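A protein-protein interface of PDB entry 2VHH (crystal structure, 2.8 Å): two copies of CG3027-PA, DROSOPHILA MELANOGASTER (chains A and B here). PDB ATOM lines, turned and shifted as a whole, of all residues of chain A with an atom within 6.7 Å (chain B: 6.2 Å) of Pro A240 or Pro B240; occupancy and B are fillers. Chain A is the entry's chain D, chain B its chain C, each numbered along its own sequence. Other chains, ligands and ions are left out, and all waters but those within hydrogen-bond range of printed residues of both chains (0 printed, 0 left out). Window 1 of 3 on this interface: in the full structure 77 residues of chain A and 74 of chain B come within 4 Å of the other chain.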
ATOM      1  N   GLY A 236      -5.801 -21.659  26.912  1.00  0.00           N
ATOM      2  CA  GLY A 236      -4.686 -22.311  26.221  1.00  0.00           C
ATOM      3  C   GLY A 236      -5.035 -23.749  25.876  1.00  0.00           C
ATOM      4  O   GLY A 236      -4.406 -24.377  25.018  1.00  0.00           O
ATOM      5  N   ARG A 237      -6.047 -24.257  26.578  1.00  0.00           N
ATOM      6  CA  ARG A 237      -6.704 -25.539  26.312  1.00  0.00           C
ATOM      7  C   ARG A 237      -7.061 -25.737  24.831  1.00  0.00           C
ATOM      8  O   ARG A 237      -6.959 -26.849  24.306  1.00  0.00           O
ATOM      9  CB  ARG A 237      -7.975 -25.571  27.140  1.00  0.00           C
ATOM     10  CG  ARG A 237      -8.781 -26.818  27.102  1.00  0.00           C
ATOM     11  CD  ARG A 237     -10.211 -26.463  27.464  1.00  0.00           C
ATOM     12  NE  ARG A 237     -10.231 -25.148  28.083  1.00  0.00           N
ATOM     13  CZ  ARG A 237     -11.295 -24.369  28.184  1.00  0.00           C
ATOM     14  NH1 ARG A 237     -12.479 -24.758  27.724  1.00  0.00           N
ATOM     15  NH2 ARG A 237     -11.161 -23.188  28.755  1.00  0.00           N
ATOM     16  N   HIS A 238      -7.479 -24.658  24.169  1.00  0.00           N
ATOM     17  CA  HIS A 238      -7.920 -24.735  22.784  1.00  0.00           C
ATOM     18  C   HIS A 238      -6.778 -24.680  21.776  1.00  0.00           C
ATOM     19  O   HIS A 238      -7.026 -24.635  20.566  1.00  0.00           O
ATOM     20  CB  HIS A 238      -8.903 -23.612  22.467  1.00  0.00           C
ATOM     21  CG  HIS A 238     -10.035 -23.498  23.435  1.00  0.00           C
ATOM     22  ND1 HIS A 238     -10.830 -24.568  23.779  1.00  0.00           N
ATOM     23  CD2 HIS A 238     -10.527 -22.434  24.107  1.00  0.00           C
ATOM     24  CE1 HIS A 238     -11.754 -24.173  24.636  1.00  0.00           C
ATOM     25  NE2 HIS A 238     -11.592 -22.883  24.852  1.00  0.00           N
ATOM     26  N   HIS A 239      -5.540 -24.675  22.259  1.00  0.00           N
ATOM     27  CA  HIS A 239      -4.397 -24.521  21.370  1.00  0.00           C
ATOM     28  C   HIS A 239      -3.440 -25.697  21.421  1.00  0.00           C
ATOM     29  O   HIS A 239      -2.597 -25.779  22.315  1.00  0.00           O
ATOM     30  CB  HIS A 239      -3.670 -23.200  21.636  1.00  0.00           C
ATOM     31  CG  HIS A 239      -4.433 -22.001  21.172  1.00  0.00           C
ATOM     32  ND1 HIS A 239      -5.483 -21.469  21.886  1.00  0.00           N
ATOM     33  CD2 HIS A 239      -4.309 -21.244  20.060  1.00  0.00           C
ATOM     34  CE1 HIS A 239      -5.965 -20.425  21.241  1.00  0.00           C
ATOM     35  NE2 HIS A 239      -5.277 -20.273  20.123  1.00  0.00           N
ATOM     36  N   PRO A 240      -3.576 -26.619  20.456  1.00  0.00           N
ATOM     37  CA  PRO A 240      -2.737 -27.813  20.405  1.00  0.00           C
ATOM     38  C   PRO A 240      -1.245 -27.490  20.411  1.00  0.00           C
ATOM     39  O   PRO A 240      -0.448 -28.219  21.010  1.00  0.00           O
ATOM     40  CB  PRO A 240      -3.158 -28.472  19.086  1.00  0.00           C
ATOM     41  CG  PRO A 240      -4.563 -28.020  18.889  1.00  0.00           C
ATOM     42  CD  PRO A 240      -4.560 -26.599  19.358  1.00  0.00           C
ATOM     43  N   GLN A 241      -0.878 -26.390  19.773  1.00  0.00           N
ATOM     44  CA  GLN A 241       0.516 -26.003  19.693  1.00  0.00           C
ATOM     45  C   GLN A 241       1.053 -25.576  21.077  1.00  0.00           C
ATOM     46  O   GLN A 241       2.242 -25.743  21.366  1.00  0.00           O
ATOM     47  CB  GLN A 241       0.728 -24.952  18.593  1.00  0.00           C
ATOM     48  CG  GLN A 241       0.282 -23.545  18.926  1.00  0.00           C
ATOM     49  CD  GLN A 241      -1.211 -23.317  18.821  1.00  0.00           C
ATOM     50  OE1 GLN A 241      -2.023 -24.228  18.999  1.00  0.00           O
ATOM     51  NE2 GLN A 241      -1.585 -22.075  18.537  1.00  0.00           N
ATOM     52  N   ASN A 242       0.171 -25.062  21.932  1.00  0.00           N
ATOM     53  CA  ASN A 242       0.529 -24.736  23.307  1.00  0.00           C
ATOM     54  C   ASN A 242       0.838 -26.009  24.101  1.00  0.00           C
ATOM     55  O   ASN A 242       1.918 -26.140  24.701  1.00  0.00           O
ATOM     56  CB  ASN A 242      -0.590 -23.931  23.966  1.00  0.00           C
ATOM     57  CG  ASN A 242      -0.177 -23.315  25.298  1.00  0.00           C
ATOM     58  OD1 ASN A 242       0.947 -22.821  25.463  1.00  0.00           O
ATOM     59  ND2 ASN A 242      -1.103 -23.323  26.252  1.00  0.00           N
ATOM     60  N   TRP A 243      -0.101 -26.951  24.085  1.00  0.00           N
ATOM     61  CA  TRP A 243       0.121 -28.278  24.640  1.00  0.00           C
ATOM     62  C   TRP A 243       1.425 -28.851  24.116  1.00  0.00           C
ATOM     63  O   TRP A 243       2.226 -29.372  24.897  1.00  0.00           O
ATOM     64  CB  TRP A 243      -1.014 -29.214  24.258  1.00  0.00           C
ATOM     65  CG  TRP A 243      -2.334 -28.891  24.895  1.00  0.00           C
ATOM     66  CD1 TRP A 243      -3.436 -28.376  24.278  1.00  0.00           C
ATOM     67  CD2 TRP A 243      -2.699 -29.075  26.273  1.00  0.00           C
ATOM     68  NE1 TRP A 243      -4.463 -28.226  25.180  1.00  0.00           N
ATOM     69  CE2 TRP A 243      -4.038 -28.648  26.410  1.00  0.00           C
ATOM     70  CE3 TRP A 243      -2.023 -29.557  27.402  1.00  0.00           C
ATOM     71  CZ2 TRP A 243      -4.715 -28.682  27.632  1.00  0.00           C
ATOM     72  CZ3 TRP A 243      -2.702 -29.597  28.618  1.00  0.00           C
ATOM     73  CH2 TRP A 243      -4.033 -29.159  28.721  1.00  0.00           C
ATOM     74  N   MET A 244       1.647 -28.730  22.802  1.00  0.00           N
ATOM     75  CA  MET A 244       2.794 -29.357  22.141  1.00  0.00           C
ATOM     76  C   MET A 244       4.117 -28.831  22.682  1.00  0.00           C
ATOM     77  O   MET A 244       5.057 -29.602  22.910  1.00  0.00           O
ATOM     78  CB  MET A 244       2.716 -29.175  20.616  1.00  0.00           C
ATOM     79  CG  MET A 244       3.775 -29.931  19.778  1.00  0.00           C
ATOM     80  SD  MET A 244       3.425 -29.889  17.990  1.00  0.00           S
ATOM     81  CE  MET A 244       5.039 -30.117  17.247  1.00  0.00           C
ATOM     82  N   MET A 245       4.192 -27.522  22.896  1.00  0.00           N
ATOM     83  CA  MET A 245       5.462 -26.925  23.279  1.00  0.00           C
ATOM     84  C   MET A 245       5.856 -27.314  24.707  1.00  0.00           C
ATOM     85  O   MET A 245       7.033 -27.558  24.979  1.00  0.00           O
ATOM     86  CB  MET A 245       5.496 -25.412  23.039  1.00  0.00           C
ATOM     87  CG  MET A 245       6.902 -24.812  23.148  1.00  0.00           C
ATOM     88  SD  MET A 245       8.135 -25.459  21.975  1.00  0.00           S
ATOM     89  CE  MET A 245       9.643 -25.179  22.881  1.00  0.00           C
ATOM     90  N   ASN A 275      -7.055 -35.055  24.295  1.00  0.00           N
ATOM     91  CA  ASN A 275      -6.247 -35.132  23.093  1.00  0.00           C
ATOM     92  C   ASN A 275      -4.793 -34.752  23.340  1.00  0.00           C
ATOM     93  O   ASN A 275      -3.877 -35.380  22.808  1.00  0.00           O
ATOM     94  CB  ASN A 275      -6.841 -34.242  22.014  1.00  0.00           C
ATOM     95  CG  ASN A 275      -6.188 -34.457  20.660  1.00  0.00           C
ATOM     96  OD1 ASN A 275      -5.280 -33.718  20.263  1.00  0.00           O
ATOM     97  ND2 ASN A 275      -6.625 -35.493  19.961  1.00  0.00           N
ATOM     98  N   ALA A 276      -4.605 -33.719  24.151  1.00  0.00           N
ATOM     99  CA  ALA A 276      -3.289 -33.221  24.511  1.00  0.00           C
ATOM    100  C   ALA A 276      -2.438 -34.318  25.117  1.00  0.00           C
ATOM    101  O   ALA A 276      -1.272 -34.481  24.752  1.00  0.00           O
ATOM    102  CB  ALA A 276      -3.429 -32.101  25.481  1.00  0.00           C
ATOM    103  N   ALA A 279      -1.541 -36.895  22.204  1.00  0.00           N
ATOM    104  CA  ALA A 279      -0.613 -36.398  21.189  1.00  0.00           C
ATOM    105  C   ALA A 279       0.801 -36.189  21.723  1.00  0.00           C
ATOM    106  O   ALA A 279       1.780 -36.417  21.013  1.00  0.00           O
ATOM    107  CB  ALA A 279      -1.129 -35.129  20.601  1.00  0.00           C
ATOM    108  N   ASN A 280       0.895 -35.770  22.981  1.00  0.00           N
ATOM    109  CA  ASN A 280       2.179 -35.437  23.579  1.00  0.00           C
ATOM    110  C   ASN A 280       2.695 -36.492  24.546  1.00  0.00           C
ATOM    111  O   ASN A 280       3.749 -36.310  25.157  1.00  0.00           O
ATOM    112  CB  ASN A 280       2.105 -34.105  24.305  1.00  0.00           C
ATOM    113  CG  ASN A 280       1.531 -33.005  23.457  1.00  0.00           C
ATOM    114  OD1 ASN A 280       2.214 -32.446  22.604  1.00  0.00           O
ATOM    115  ND2 ASN A 280       0.272 -32.673  23.700  1.00  0.00           N
ATOM    116  N   TYR A 282       1.924 -37.432  27.589  1.00  0.00           N
ATOM    117  CA  TYR A 282       2.122 -37.076  28.977  1.00  0.00           C
ATOM    118  C   TYR A 282       0.771 -37.037  29.680  1.00  0.00           C
ATOM    119  O   TYR A 282      -0.247 -37.326  29.057  1.00  0.00           O
ATOM    120  CB  TYR A 282       2.907 -35.772  29.118  1.00  0.00           C
ATOM    121  CG  TYR A 282       2.339 -34.563  28.426  1.00  0.00           C
ATOM    122  CD1 TYR A 282       3.177 -33.659  27.790  1.00  0.00           C
ATOM    123  CD2 TYR A 282       0.964 -34.302  28.415  1.00  0.00           C
ATOM    124  CE1 TYR A 282       2.665 -32.528  27.156  1.00  0.00           C
ATOM    125  CE2 TYR A 282       0.443 -33.174  27.774  1.00  0.00           C
ATOM    126  CZ  TYR A 282       1.304 -32.293  27.156  1.00  0.00           C
ATOM    127  OH  TYR A 282       0.808 -31.175  26.539  1.00  0.00           O
ATOM    128  N   TYR A 366       7.530 -28.483  10.347  1.00  0.00           N
ATOM    129  CA  TYR A 366       6.485 -27.650  10.886  1.00  0.00           C
ATOM    130  C   TYR A 366       6.959 -26.270  11.327  1.00  0.00           C
ATOM    131  O   TYR A 366       6.217 -25.295  11.195  1.00  0.00           O
ATOM    132  CB  TYR A 366       5.741 -28.409  11.986  1.00  0.00           C
ATOM    133  CG  TYR A 366       4.895 -29.503  11.390  1.00  0.00           C
ATOM    134  CD1 TYR A 366       5.323 -30.827  11.397  1.00  0.00           C
ATOM    135  CD2 TYR A 366       3.689 -29.205  10.756  1.00  0.00           C
ATOM    136  CE1 TYR A 366       4.552 -31.826  10.817  1.00  0.00           C
ATOM    137  CE2 TYR A 366       2.926 -30.184  10.188  1.00  0.00           C
ATOM    138  CZ  TYR A 366       3.358 -31.488  10.219  1.00  0.00           C
ATOM    139  OH  TYR A 366       2.583 -32.456   9.641  1.00  0.00           O
ATOM    140  N   PHE A 370       5.223 -23.081   9.662  1.00  0.00           N
ATOM    141  CA  PHE A 370       4.625 -22.083  10.542  1.00  0.00           C
ATOM    142  C   PHE A 370       5.259 -20.714  10.310  1.00  0.00           C
ATOM    143  O   PHE A 370       4.603 -19.681  10.465  1.00  0.00           O
ATOM    144  CB  PHE A 370       4.778 -22.497  12.014  1.00  0.00           C
ATOM    145  CG  PHE A 370       3.807 -23.568  12.472  1.00  0.00           C
ATOM    146  CD1 PHE A 370       3.568 -23.760  13.831  1.00  0.00           C
ATOM    147  CD2 PHE A 370       3.136 -24.378  11.569  1.00  0.00           C
ATOM    148  CE1 PHE A 370       2.678 -24.751  14.284  1.00  0.00           C
ATOM    149  CE2 PHE A 370       2.251 -25.368  12.011  1.00  0.00           C
ATOM    150  CZ  PHE A 370       2.021 -25.551  13.368  1.00  0.00           C
ATOM    151  N   GLY B 236      -1.452 -39.557  10.522  1.00  0.00           N
ATOM    152  CA  GLY B 236      -1.362 -38.103  10.685  1.00  0.00           C
ATOM    153  C   GLY B 236      -2.433 -37.568  11.630  1.00  0.00           C
ATOM    154  O   GLY B 236      -2.346 -36.434  12.131  1.00  0.00           O
ATOM    155  N   ARG B 237      -3.455 -38.399  11.839  1.00  0.00           N
ATOM    156  CA  ARG B 237      -4.493 -38.232  12.854  1.00  0.00           C
ATOM    157  C   ARG B 237      -3.927 -37.835  14.220  1.00  0.00           C
ATOM    158  O   ARG B 237      -4.518 -37.022  14.931  1.00  0.00           O
ATOM    159  CB  ARG B 237      -5.148 -39.589  13.015  1.00  0.00           C
ATOM    160  CG  ARG B 237      -6.587 -39.657  13.440  1.00  0.00           C
ATOM    161  CD  ARG B 237      -6.897 -41.099  13.860  1.00  0.00           C
ATOM    162  NE  ARG B 237      -5.916 -42.033  13.306  1.00  0.00           N
ATOM    163  CZ  ARG B 237      -5.598 -43.213  13.831  1.00  0.00           C
ATOM    164  NH1 ARG B 237      -6.189 -43.658  14.938  1.00  0.00           N
ATOM    165  NH2 ARG B 237      -4.681 -43.957  13.238  1.00  0.00           N
ATOM    166  N   HIS B 238      -2.779 -38.419  14.572  1.00  0.00           N
ATOM    167  CA  HIS B 238      -2.165 -38.239  15.888  1.00  0.00           C
ATOM    168  C   HIS B 238      -1.281 -36.995  16.004  1.00  0.00           C
ATOM    169  O   HIS B 238      -0.649 -36.773  17.039  1.00  0.00           O
ATOM    170  CB  HIS B 238      -1.346 -39.476  16.271  1.00  0.00           C
ATOM    171  CG  HIS B 238      -2.114 -40.761  16.220  1.00  0.00           C
ATOM    172  ND1 HIS B 238      -3.295 -40.953  16.902  1.00  0.00           N
ATOM    173  CD2 HIS B 238      -1.852 -41.929  15.590  1.00  0.00           C
ATOM    174  CE1 HIS B 238      -3.735 -42.179  16.687  1.00  0.00           C
ATOM    175  NE2 HIS B 238      -2.877 -42.794  15.896  1.00  0.00           N
ATOM    176  N   HIS B 239      -1.239 -36.188  14.950  1.00  0.00           N
ATOM    177  CA  HIS B 239      -0.358 -35.022  14.912  1.00  0.00           C
ATOM    178  C   HIS B 239      -1.133 -33.718  14.768  1.00  0.00           C
ATOM    179  O   HIS B 239      -1.494 -33.335  13.662  1.00  0.00           O
ATOM    180  CB  HIS B 239       0.681 -35.183  13.801  1.00  0.00           C
ATOM    181  CG  HIS B 239       1.724 -36.205  14.115  1.00  0.00           C
ATOM    182  ND1 HIS B 239       1.608 -37.524  13.739  1.00  0.00           N
ATOM    183  CD2 HIS B 239       2.889 -36.110  14.799  1.00  0.00           C
ATOM    184  CE1 HIS B 239       2.662 -38.197  14.164  1.00  0.00           C
ATOM    185  NE2 HIS B 239       3.454 -37.361  14.810  1.00  0.00           N
ATOM    186  N   PRO B 240      -1.413 -33.046  15.902  1.00  0.00           N
ATOM    187  CA  PRO B 240      -2.142 -31.777  15.889  1.00  0.00           C
ATOM    188  C   PRO B 240      -1.540 -30.759  14.933  1.00  0.00           C
ATOM    189  O   PRO B 240      -2.277 -30.014  14.285  1.00  0.00           O
ATOM    190  CB  PRO B 240      -2.027 -31.297  17.336  1.00  0.00           C
ATOM    191  CG  PRO B 240      -1.902 -32.543  18.120  1.00  0.00           C
ATOM    192  CD  PRO B 240      -1.082 -33.469  17.276  1.00  0.00           C
ATOM    193  N   GLN B 241      -0.218 -30.754  14.825  1.00  0.00           N
ATOM    194  CA  GLN B 241       0.481 -29.820  13.945  1.00  0.00           C
ATOM    195  C   GLN B 241       0.191 -30.080  12.471  1.00  0.00           C
ATOM    196  O   GLN B 241       0.151 -29.139  11.686  1.00  0.00           O
ATOM    197  CB  GLN B 241       1.992 -29.784  14.233  1.00  0.00           C
ATOM    198  CG  GLN B 241       2.799 -30.981  13.800  1.00  0.00           C
ATOM    199  CD  GLN B 241       2.660 -32.177  14.705  1.00  0.00           C
ATOM    200  OE1 GLN B 241       1.645 -32.363  15.368  1.00  0.00           O
ATOM    201  NE2 GLN B 241       3.678 -33.016  14.718  1.00  0.00           N
ATOM    202  N   ASN B 242      -0.029 -31.346  12.112  1.00  0.00           N
ATOM    203  CA  ASN B 242      -0.478 -31.731  10.784  1.00  0.00           C
ATOM    204  C   ASN B 242      -1.859 -31.135  10.466  1.00  0.00           C
ATOM    205  O   ASN B 242      -2.032 -30.420   9.464  1.00  0.00           O
ATOM    206  CB  ASN B 242      -0.517 -33.251  10.687  1.00  0.00           C
ATOM    207  CG  ASN B 242      -0.510 -33.763   9.243  1.00  0.00           C
ATOM    208  OD1 ASN B 242       0.116 -33.169   8.355  1.00  0.00           O
ATOM    209  ND2 ASN B 242      -1.188 -34.894   9.015  1.00  0.00           N
ATOM    210  N   TRP B 243      -2.826 -31.409  11.338  1.00  0.00           N
ATOM    211  CA  TRP B 243      -4.151 -30.824  11.245  1.00  0.00           C
ATOM    212  C   TRP B 243      -4.061 -29.311  11.149  1.00  0.00           C
ATOM    213  O   TRP B 243      -4.762 -28.687  10.339  1.00  0.00           O
ATOM    214  CB  TRP B 243      -4.968 -31.176  12.473  1.00  0.00           C
ATOM    215  CG  TRP B 243      -5.425 -32.601  12.612  1.00  0.00           C
ATOM    216  CD1 TRP B 243      -4.960 -33.504  13.506  1.00  0.00           C
ATOM    217  CD2 TRP B 243      -6.484 -33.261  11.891  1.00  0.00           C
ATOM    218  NE1 TRP B 243      -5.637 -34.695  13.385  1.00  0.00           N
ATOM    219  CE2 TRP B 243      -6.585 -34.569  12.406  1.00  0.00           C
ATOM    220  CE3 TRP B 243      -7.353 -32.875  10.863  1.00  0.00           C
ATOM    221  CZ2 TRP B 243      -7.514 -35.497  11.925  1.00  0.00           C
ATOM    222  CZ3 TRP B 243      -8.284 -33.793  10.393  1.00  0.00           C
ATOM    223  CH2 TRP B 243      -8.353 -35.085  10.921  1.00  0.00           C
ATOM    224  N   MET B 244      -3.195 -28.720  11.974  1.00  0.00           N
ATOM    225  CA  MET B 244      -3.095 -27.263  12.055  1.00  0.00           C
ATOM    226  C   MET B 244      -2.629 -26.629  10.746  1.00  0.00           C
ATOM    227  O   MET B 244      -3.111 -25.574  10.353  1.00  0.00           O
ATOM    228  CB  MET B 244      -2.179 -26.860  13.197  1.00  0.00           C
ATOM    229  CG  MET B 244      -2.237 -25.396  13.548  1.00  0.00           C
ATOM    230  SD  MET B 244      -1.038 -25.016  14.828  1.00  0.00           S
ATOM    231  CE  MET B 244      -0.963 -23.227  14.738  1.00  0.00           C
ATOM    232  N   MET B 245      -1.701 -27.295  10.071  1.00  0.00           N
ATOM    233  CA  MET B 245      -1.104 -26.749   8.873  1.00  0.00           C
ATOM    234  C   MET B 245      -2.105 -26.739   7.712  1.00  0.00           C
ATOM    235  O   MET B 245      -2.144 -25.793   6.933  1.00  0.00           O
ATOM    236  CB  MET B 245       0.184 -27.497   8.541  1.00  0.00           C
ATOM    237  CG  MET B 245       1.087 -26.766   7.564  1.00  0.00           C
ATOM    238  SD  MET B 245       1.492 -25.089   8.072  1.00  0.00           S
ATOM    239  CE  MET B 245       1.575 -24.252   6.481  1.00  0.00           C
ATOM    240  N   ASN B 275     -11.094 -33.155  17.900  1.00  0.00           N
ATOM    241  CA  ASN B 275     -10.286 -32.032  18.393  1.00  0.00           C
ATOM    242  C   ASN B 275      -9.797 -31.151  17.253  1.00  0.00           C
ATOM    243  O   ASN B 275      -9.842 -29.934  17.335  1.00  0.00           O
ATOM    244  CB  ASN B 275      -9.098 -32.548  19.231  1.00  0.00           C
ATOM    245  CG  ASN B 275      -8.372 -31.435  20.013  1.00  0.00           C
ATOM    246  OD1 ASN B 275      -8.207 -30.317  19.549  1.00  0.00           O
ATOM    247  ND2 ASN B 275      -7.923 -31.765  21.197  1.00  0.00           N
ATOM    248  N   ALA B 279     -10.151 -27.114  17.130  1.00  0.00           N
ATOM    249  CA  ALA B 279      -8.977 -26.256  17.193  1.00  0.00           C
ATOM    250  C   ALA B 279      -8.829 -25.407  15.931  1.00  0.00           C
ATOM    251  O   ALA B 279      -8.480 -24.227  16.003  1.00  0.00           O
ATOM    252  CB  ALA B 279      -7.725 -27.103  17.433  1.00  0.00           C
ATOM    253  N   ASN B 280      -9.121 -26.009  14.781  1.00  0.00           N
ATOM    254  CA  ASN B 280      -8.872 -25.380  13.494  1.00  0.00           C
ATOM    255  C   ASN B 280     -10.098 -24.805  12.830  1.00  0.00           C
ATOM    256  O   ASN B 280     -10.008 -24.272  11.726  1.00  0.00           O
ATOM    257  CB  ASN B 280      -8.225 -26.370  12.564  1.00  0.00           C
ATOM    258  CG  ASN B 280      -6.874 -26.794  13.047  1.00  0.00           C
ATOM    259  OD1 ASN B 280      -5.897 -26.054  12.913  1.00  0.00           O
ATOM    260  ND2 ASN B 280      -6.801 -27.991  13.619  1.00  0.00           N
ATOM    261  N   GLN B 361      -3.684 -17.540  17.896  1.00  0.00           N
ATOM    262  CA  GLN B 361      -2.748 -18.664  17.763  1.00  0.00           C
ATOM    263  C   GLN B 361      -1.291 -18.349  18.066  1.00  0.00           C
ATOM    264  O   GLN B 361      -0.553 -19.222  18.507  1.00  0.00           O
ATOM    265  CB  GLN B 361      -2.851 -19.321  16.396  1.00  0.00           C
ATOM    266  CG  GLN B 361      -3.714 -20.550  16.385  1.00  0.00           C
ATOM    267  CD  GLN B 361      -3.946 -21.074  14.989  1.00  0.00           C
ATOM    268  OE1 GLN B 361      -3.855 -20.334  14.006  1.00  0.00           O
ATOM    269  NE2 GLN B 361      -4.240 -22.355  14.889  1.00  0.00           N
ATOM    270  N   PHE B 370       9.401 -23.806  17.905  1.00  0.00           N
ATOM    271  CA  PHE B 370       9.590 -25.091  17.237  1.00  0.00           C
ATOM    272  C   PHE B 370      10.950 -25.164  16.529  1.00  0.00           C
ATOM    273  O   PHE B 370      11.535 -26.244  16.409  1.00  0.00           O
ATOM    274  CB  PHE B 370       8.445 -25.381  16.259  1.00  0.00           C
ATOM    275  CG  PHE B 370       7.148 -25.795  16.921  1.00  0.00           C
ATOM    276  CD1 PHE B 370       6.056 -26.170  16.146  1.00  0.00           C
ATOM    277  CD2 PHE B 370       7.018 -25.820  18.305  1.00  0.00           C
ATOM    278  CE1 PHE B 370       4.852 -26.546  16.739  1.00  0.00           C
ATOM    279  CE2 PHE B 370       5.820 -26.196  18.911  1.00  0.00           C
ATOM    280  CZ  PHE B 370       4.734 -26.560  18.129  1.00  0.00           C
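OD1 of Asn B242 is in hydrogen-bond range of OH of Tyr A366 (2.9 Å). The side-chain amide nitrogen (ND2) of Asn B275 lies close to the side-chain amide oxygen (OD1) of Asn A275. NE2 of Gln A241 is in hydrogen-bond range of O of Gln B361, 3.0 Å away.
NH2 of Arg B237 sits at hydrogen-bond distance from NE2 of His B238, at 3.4 Å.
Gln B361 touches His A239 (CG to CD2, 3.8 Å). Pro B240 touches Pro A240 (CB to CB, 3.5 Å). CG of Pro A240 touches CB of Ala B279, at 3.6 Å. Met A244 touches Phe B370. Met A245 touches Phe B370. His B238 touches Ala A279 (O to CB, 3.95 Å). O of Gln B241 touches CE2 of Tyr A366, at 3.3 Å. CZ of Phe A370 touches SD of Met B244 (3.4 Å). Phe A370 touches Met B245. Phe A370 touches Phe B370.
Arg A237 touches none of the printed residues of chain B. Of the printed residues of chain B, Gln A241 touches Gln B361 (3.0 Å). Of the printed residues of chain B, Ala A279 touches His B238 (3.95 Å) and Pro B240 (3.7 Å). Pro B240 touches just these residues of chain A: Pro A240 and Ala A279. Printed residues of chain A within 4 Å of Ala B279: Pro A240 (3.6 Å). Of the printed residues of chain A, Phe B370 touches Met A244 (3.6 Å), Met A245 (3.9 Å) and Phe A370 (3.7 Å). The nearest residue of chain B that does not touch Pro A240 is Asn B275 (4.4 Å). The nearest residue of chain A that does not touch Pro B240 is Asn A275 (4.2 Å). The nearest printed residue of chain B that does not touch Ala A279 is His B239 (5.7 Å).
Of the 17 printed residues of chain A, 9 touch a printed residue of chain B. Of the 15 printed residues of chain B, 10 touch a printed residue of chain A. Hydrophobic or aromatic side chains of chain B that line the printed part of chain A: Pro B240, Met B244, Met B245, Ala B279 and Phe B370. Among the printed residues, no Asp or Glu carboxylate lies within 4 Å of a Lys or Arg side-chain nitrogen of the other chain.
Pro A240 touches its own counterpart, Pro B240. Pro A240 touches Ala B279, and with the chains exchanged Ala A279 touches Pro B240. Asn A275 touches its own counterpart, Asn B275. Phe B370 touches its own counterpart, Phe A370. Positions printed for both chains: 236, 237, 238, 239, 240, 241, 242, 243, 244, 245, 275, 279, 280 and 370.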
